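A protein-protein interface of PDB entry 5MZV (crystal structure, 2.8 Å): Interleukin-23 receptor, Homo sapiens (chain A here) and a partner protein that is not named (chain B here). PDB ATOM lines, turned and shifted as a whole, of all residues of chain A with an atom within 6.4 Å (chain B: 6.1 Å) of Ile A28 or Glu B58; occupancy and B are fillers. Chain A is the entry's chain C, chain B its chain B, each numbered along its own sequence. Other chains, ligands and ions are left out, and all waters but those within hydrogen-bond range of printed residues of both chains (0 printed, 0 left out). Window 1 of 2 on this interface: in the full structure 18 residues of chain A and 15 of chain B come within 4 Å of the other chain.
The backbone NH of Arg B57 lies within hydrogen-bond range of the backbone carbonyl oxygen of Glu A111 (3.2 Å). The guanidinium group (NH1) of Arg B57 is in hydrogen-bond range of the side-chain hydroxyl (OG1) of Thr A112 (2.8 Å). O of Arg B57 lies within hydrogen-bond range of N of Leu A113, 2.8 Å away. OE1 of Glu B58 lies within hydrogen-bond range of N of Asn A29 (3.2 Å). OD1 of Asn A29 lies close to O of Glu B59, at 2.7 Å. The side-chain amino group of Lys B164 is in hydrogen-bond range of the backbone carbonyl oxygen of Gly A24. The backbone carbonyl oxygen (O) of Asn A27 lies within hydrogen-bond range of the side-chain amino group (NZ) of Lys B164 (3.3 Å).
The guanidinium group (NH2) of Arg B57 is in salt-bridge range of the side-chain carboxylate (OE2) of Glu B59 (3.0 Å). The side-chain carboxylate (OE1) of Glu B58 lies within salt-bridge range of the side-chain amino group (NZ) of Lys B164 (2.9 Å). The backbone NH (N) of Gly A24 lies within hydrogen-bond range of the side-chain amide oxygen (OD1) of Asn A27.
Lys B164 touches Ile A25 (CD to O, 3.8 Å). C of Thr A26 touches CD2 of Leu B161, 3.9 Å away. N of Asn A27 touches CD2 of Leu B161, at 3.7 Å. OE2 of Glu B58 touches CD1 of Ile A28 (3.6 Å). CB of Gln B157 touches CG1 of Ile A28 (3.7 Å). CB of Leu B160 touches CD1 of Ile A28, at 3.9 Å. CD2 of Leu B161 touches CD1 of Ile A28, at 3.9 Å. Ser A31 touches Glu B59 (OG to CB, 3.4 Å). Glu A111 touches Leu B56.
Of chain B, only Glu B58 (3.6 Å), Gln B157 (3.7 Å), Leu B160 (3.9 Å) and Leu B161 (3.9 Å) come within 4 Å of Ile A28. Printed residues of chain A within 4 Å of Glu B58: Ile A28 and Asn A29. Printed residues of chain A within 4 Å of Arg B57: Glu A111 (3.2 Å), Thr A112 (2.8 Å) and Leu A113 (2.8 Å). Of the printed residues of chain B, Gly A24 touches Lys B164. Trp B156 touches none of the printed residues of chain A.
Of the 10 printed residues of chain B, 8 touch a printed residue of chain A. Hydrophobic or aromatic side chains of chain B that line the printed part of chain A: Leu B56, Leu B160 and Leu B161. Among the printed residues, no Asp or Glu carboxylate lies within 4 Å of a Lys or Arg side-chain nitrogen of the other chain.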
ATOM      1  N   GLY A  24      13.593  21.121  10.659  1.00  0.00           N
ATOM      2  CA  GLY A  24      12.483  20.250  10.999  1.00  0.00           C
ATOM      3  C   GLY A  24      12.129  19.279   9.890  1.00  0.00           C
ATOM      4  O   GLY A  24      12.964  18.486   9.452  1.00  0.00           O
ATOM      5  N   ILE A  25      10.882  19.348   9.430  1.00  0.00           N
ATOM      6  CA  ILE A  25      10.382  18.429   8.412  1.00  0.00           C
ATOM      7  C   ILE A  25      10.353  19.127   7.059  1.00  0.00           C
ATOM      8  O   ILE A  25      10.570  18.496   6.019  1.00  0.00           O
ATOM      9  CB  ILE A  25       8.988  17.888   8.784  1.00  0.00           C
ATOM     10  CG1 ILE A  25       8.440  17.025   7.644  1.00  0.00           C
ATOM     11  CG2 ILE A  25       8.030  19.033   9.111  1.00  0.00           C
ATOM     12  CD1 ILE A  25       7.118  16.373   7.951  1.00  0.00           C
ATOM     13  N   THR A  26      10.076  20.429   7.060  1.00  0.00           N
ATOM     14  CA  THR A  26       9.991  21.210   5.833  1.00  0.00           C
ATOM     15  C   THR A  26      11.273  21.975   5.535  1.00  0.00           C
ATOM     16  O   THR A  26      11.267  22.867   4.680  1.00  0.00           O
ATOM     17  CB  THR A  26       8.818  22.190   5.911  1.00  0.00           C
ATOM     18  OG1 THR A  26       8.898  22.943   7.128  1.00  0.00           O
ATOM     19  CG2 THR A  26       7.492  21.446   5.851  1.00  0.00           C
ATOM     20  N   ASN A  27      12.370  21.649   6.212  1.00  0.00           N
ATOM     21  CA  ASN A  27      13.598  22.410   6.059  1.00  0.00           C
ATOM     22  C   ASN A  27      14.768  21.561   6.525  1.00  0.00           C
ATOM     23  O   ASN A  27      14.635  20.749   7.443  1.00  0.00           O
ATOM     24  CB  ASN A  27      13.545  23.713   6.864  1.00  0.00           C
ATOM     25  CG  ASN A  27      13.491  23.465   8.360  1.00  0.00           C
ATOM     26  OD1 ASN A  27      12.423  23.219   8.922  1.00  0.00           O
ATOM     27  ND2 ASN A  27      14.646  23.525   9.012  1.00  0.00           N
ATOM     28  N   ILE A  28      15.907  21.761   5.884  1.00  0.00           N
ATOM     29  CA  ILE A  28      17.157  21.138   6.299  1.00  0.00           C
ATOM     30  C   ILE A  28      17.803  22.015   7.358  1.00  0.00           C
ATOM     31  O   ILE A  28      17.721  23.249   7.302  1.00  0.00           O
ATOM     32  CB  ILE A  28      18.094  20.934   5.096  1.00  0.00           C
ATOM     33  CG1 ILE A  28      17.414  20.066   4.030  1.00  0.00           C
ATOM     34  CG2 ILE A  28      19.413  20.314   5.542  1.00  0.00           C
ATOM     35  CD1 ILE A  28      17.038  18.674   4.502  1.00  0.00           C
ATOM     36  N   ASN A  29      18.448  21.379   8.330  1.00  0.00           N
ATOM     37  CA  ASN A  29      19.113  22.077   9.425  1.00  0.00           C
ATOM     38  C   ASN A  29      20.603  21.763   9.339  1.00  0.00           C
ATOM     39  O   ASN A  29      21.051  20.710   9.805  1.00  0.00           O
ATOM     40  CB  ASN A  29      18.531  21.664  10.773  1.00  0.00           C
ATOM     41  CG  ASN A  29      18.848  22.659  11.870  1.00  0.00           C
ATOM     42  OD1 ASN A  29      19.965  22.697  12.386  1.00  0.00           O
ATOM     43  ND2 ASN A  29      17.862  23.474  12.233  1.00  0.00           N
ATOM     44  N   CYS A  30      21.363  22.671   8.734  1.00  0.00           N
ATOM     45  CA  CYS A  30      22.797  22.473   8.623  1.00  0.00           C
ATOM     46  C   CYS A  30      23.474  22.677   9.974  1.00  0.00           C
ATOM     47  O   CYS A  30      22.974  23.387  10.850  1.00  0.00           O
ATOM     48  CB  CYS A  30      23.384  23.423   7.582  1.00  0.00           C
ATOM     49  SG  CYS A  30      22.713  23.156   5.926  1.00  0.00           S
ATOM     50  N   SER A  31      24.625  22.028  10.136  1.00  0.00           N
ATOM     51  CA  SER A  31      25.389  22.073  11.374  1.00  0.00           C
ATOM     52  C   SER A  31      26.862  22.290  11.020  1.00  0.00           C
ATOM     53  O   SER A  31      27.750  21.528  11.390  1.00  0.00           O
ATOM     54  CB  SER A  31      25.184  20.793  12.178  1.00  0.00           C
ATOM     55  OG  SER A  31      23.825  20.393  12.178  1.00  0.00           O
ATOM     56  N   GLU A 111      25.287   9.153  10.187  1.00  0.00           N
ATOM     57  CA  GLU A 111      26.102  10.298   9.813  1.00  0.00           C
ATOM     58  C   GLU A 111      25.275  11.567   9.967  1.00  0.00           C
ATOM     59  O   GLU A 111      24.136  11.638   9.494  1.00  0.00           O
ATOM     60  CB  GLU A 111      26.607  10.148   8.380  1.00  0.00           C
ATOM     61  CG  GLU A 111      27.473   8.920   8.167  1.00  0.00           C
ATOM     62  CD  GLU A 111      27.974   8.794   6.739  1.00  0.00           C
ATOM     63  OE1 GLU A 111      27.562   9.608   5.884  1.00  0.00           O
ATOM     64  OE2 GLU A 111      28.780   7.877   6.470  1.00  0.00           O
ATOM     65  N   THR A 112      25.838  12.558  10.650  1.00  0.00           N
ATOM     66  CA  THR A 112      25.142  13.813  10.912  1.00  0.00           C
ATOM     67  C   THR A 112      25.395  14.775   9.758  1.00  0.00           C
ATOM     68  O   THR A 112      26.548  15.109   9.462  1.00  0.00           O
ATOM     69  CB  THR A 112      25.609  14.421  12.233  1.00  0.00           C
ATOM     70  OG1 THR A 112      25.430  13.468  13.290  1.00  0.00           O
ATOM     71  CG2 THR A 112      24.824  15.685  12.554  1.00  0.00           C
ATOM     72  N   LEU A 113      24.321  15.216   9.109  1.00  0.00           N
ATOM     73  CA  LEU A 113      24.446  16.167   8.013  1.00  0.00           C
ATOM     74  C   LEU A 113      25.133  17.439   8.488  1.00  0.00           C
ATOM     75  O   LEU A 113      24.749  18.026   9.504  1.00  0.00           O
ATOM     76  CB  LEU A 113      23.068  16.502   7.446  1.00  0.00           C
ATOM     77  CG  LEU A 113      23.054  17.536   6.318  1.00  0.00           C
ATOM     78  CD1 LEU A 113      23.594  16.941   5.028  1.00  0.00           C
ATOM     79  CD2 LEU A 113      21.656  18.083   6.119  1.00  0.00           C
ATOM     80  N   LEU B  56      20.234   9.230   7.473  1.00  0.00           N
ATOM     81  CA  LEU B  56      20.979  10.472   7.629  1.00  0.00           C
ATOM     82  C   LEU B  56      20.237  11.334   8.636  1.00  0.00           C
ATOM     83  O   LEU B  56      19.029  11.546   8.494  1.00  0.00           O
ATOM     84  CB  LEU B  56      21.114  11.208   6.290  1.00  0.00           C
ATOM     85  CG  LEU B  56      22.117  12.362   6.251  1.00  0.00           C
ATOM     86  CD1 LEU B  56      23.537  11.821   6.227  1.00  0.00           C
ATOM     87  CD2 LEU B  56      21.866  13.264   5.056  1.00  0.00           C
ATOM     88  N   ARG B  57      20.947  11.821   9.651  1.00  0.00           N
ATOM     89  CA  ARG B  57      20.335  12.600  10.720  1.00  0.00           C
ATOM     90  C   ARG B  57      20.793  14.052  10.653  1.00  0.00           C
ATOM     91  O   ARG B  57      21.711  14.413   9.912  1.00  0.00           O
ATOM     92  CB  ARG B  57      20.662  12.003  12.095  1.00  0.00           C
ATOM     93  CG  ARG B  57      22.081  12.248  12.588  1.00  0.00           C
ATOM     94  CD  ARG B  57      22.239  11.811  14.036  1.00  0.00           C
ATOM     95  NE  ARG B  57      21.586  12.734  14.962  1.00  0.00           N
ATOM     96  CZ  ARG B  57      22.144  13.841  15.440  1.00  0.00           C
ATOM     97  NH1 ARG B  57      23.376  14.183  15.086  1.00  0.00           N
ATOM     98  NH2 ARG B  57      21.468  14.613  16.277  1.00  0.00           N
ATOM     99  N   GLU B  58      20.136  14.887  11.455  1.00  0.00           N
ATOM    100  CA  GLU B  58      20.418  16.313  11.495  1.00  0.00           C
ATOM    101  C   GLU B  58      20.257  16.822  12.919  1.00  0.00           C
ATOM    102  O   GLU B  58      19.441  16.311  13.689  1.00  0.00           O
ATOM    103  CB  GLU B  58      19.482  17.101  10.572  1.00  0.00           C
ATOM    104  CG  GLU B  58      19.253  16.469   9.212  1.00  0.00           C
ATOM    105  CD  GLU B  58      18.186  17.191   8.415  1.00  0.00           C
ATOM    106  OE1 GLU B  58      17.743  18.275   8.855  1.00  0.00           O
ATOM    107  OE2 GLU B  58      17.780  16.668   7.356  1.00  0.00           O
ATOM    108  N   GLU B  59      21.039  17.841  13.260  1.00  0.00           N
ATOM    109  CA  GLU B  59      20.885  18.517  14.539  1.00  0.00           C
ATOM    110  C   GLU B  59      19.678  19.446  14.485  1.00  0.00           C
ATOM    111  O   GLU B  59      19.585  20.308  13.604  1.00  0.00           O
ATOM    112  CB  GLU B  59      22.146  19.309  14.882  1.00  0.00           C
ATOM    113  CG  GLU B  59      23.359  18.445  15.180  1.00  0.00           C
ATOM    114  CD  GLU B  59      23.355  17.898  16.596  1.00  0.00           C
ATOM    115  OE1 GLU B  59      23.162  18.696  17.539  1.00  0.00           O
ATOM    116  OE2 GLU B  59      23.542  16.674  16.766  1.00  0.00           O
ATOM    117  N   GLY B  60      18.754  19.271  15.426  1.00  0.00           N
ATOM    118  CA  GLY B  60      17.555  20.088  15.464  1.00  0.00           C
ATOM    119  C   GLY B  60      16.706  19.852  16.696  1.00  0.00           C
ATOM    120  O   GLY B  60      15.694  20.523  16.900  1.00  0.00           O
ATOM    121  N   TRP B 156      19.810  20.341  -3.943  1.00  0.00           N
ATOM    122  CA  TRP B 156      20.487  19.310  -3.163  1.00  0.00           C
ATOM    123  C   TRP B 156      19.673  18.880  -1.948  1.00  0.00           C
ATOM    124  O   TRP B 156      19.839  17.756  -1.463  1.00  0.00           O
ATOM    125  CB  TRP B 156      21.869  19.800  -2.729  1.00  0.00           C
ATOM    126  CG  TRP B 156      21.852  20.950  -1.763  1.00  0.00           C
ATOM    127  CD1 TRP B 156      21.864  22.277  -2.072  1.00  0.00           C
ATOM    128  CD2 TRP B 156      21.835  20.872  -0.329  1.00  0.00           C
ATOM    129  NE1 TRP B 156      21.853  23.031  -0.924  1.00  0.00           N
ATOM    130  CE2 TRP B 156      21.836  22.193   0.159  1.00  0.00           C
ATOM    131  CE3 TRP B 156      21.817  19.815   0.586  1.00  0.00           C
ATOM    132  CZ2 TRP B 156      21.817  22.486   1.520  1.00  0.00           C
ATOM    133  CZ3 TRP B 156      21.801  20.111   1.940  1.00  0.00           C
ATOM    134  CH2 TRP B 156      21.802  21.435   2.392  1.00  0.00           C
ATOM    135  N   GLN B 157      18.790  19.745  -1.448  1.00  0.00           N
ATOM    136  CA  GLN B 157      18.001  19.410  -0.267  1.00  0.00           C
ATOM    137  C   GLN B 157      16.842  18.474  -0.583  1.00  0.00           C
ATOM    138  O   GLN B 157      16.388  17.738   0.299  1.00  0.00           O
ATOM    139  CB  GLN B 157      17.442  20.683   0.369  1.00  0.00           C
ATOM    140  CG  GLN B 157      18.487  21.678   0.818  1.00  0.00           C
ATOM    141  CD  GLN B 157      17.869  22.977   1.284  1.00  0.00           C
ATOM    142  OE1 GLN B 157      16.786  23.355   0.839  1.00  0.00           O
ATOM    143  NE2 GLN B 157      18.552  23.666   2.188  1.00  0.00           N
ATOM    144  N   LEU B 160      16.398  14.755   0.308  1.00  0.00           N
ATOM    145  CA  LEU B 160      16.246  14.591   1.750  1.00  0.00           C
ATOM    146  C   LEU B 160      14.876  15.077   2.211  1.00  0.00           C
ATOM    147  O   LEU B 160      14.258  14.465   3.089  1.00  0.00           O
ATOM    148  CB  LEU B 160      17.360  15.339   2.482  1.00  0.00           C
ATOM    149  CG  LEU B 160      18.780  15.182   1.915  1.00  0.00           C
ATOM    150  CD1 LEU B 160      19.791  15.956   2.754  1.00  0.00           C
ATOM    151  CD2 LEU B 160      19.179  13.712   1.815  1.00  0.00           C
ATOM    152  N   LEU B 161      14.385  16.173   1.626  1.00  0.00           N
ATOM    153  CA  LEU B 161      13.067  16.683   1.990  1.00  0.00           C
ATOM    154  C   LEU B 161      11.962  15.740   1.530  1.00  0.00           C
ATOM    155  O   LEU B 161      11.013  15.477   2.277  1.00  0.00           O
ATOM    156  CB  LEU B 161      12.856  18.075   1.389  1.00  0.00           C
ATOM    157  CG  LEU B 161      13.731  19.215   1.915  1.00  0.00           C
ATOM    158  CD1 LEU B 161      13.513  20.470   1.085  1.00  0.00           C
ATOM    159  CD2 LEU B 161      13.442  19.495   3.378  1.00  0.00           C
ATOM    160  N   LYS B 164      11.736  12.987   3.953  1.00  0.00           N
ATOM    161  CA  LYS B 164      11.145  13.473   5.197  1.00  0.00           C
ATOM    162  C   LYS B 164       9.635  13.615   5.068  1.00  0.00           C
ATOM    163  O   LYS B 164       8.875  13.060   5.869  1.00  0.00           O
ATOM    164  CB  LYS B 164      11.762  14.815   5.583  1.00  0.00           C
ATOM    165  CG  LYS B 164      13.050  14.739   6.376  1.00  0.00           C
ATOM    166  CD  LYS B 164      13.453  16.145   6.802  1.00  0.00           C
ATOM    167  CE  LYS B 164      14.708  16.168   7.646  1.00  0.00           C
ATOM    168  NZ  LYS B 164      15.004  17.557   8.098  1.00  0.00           N
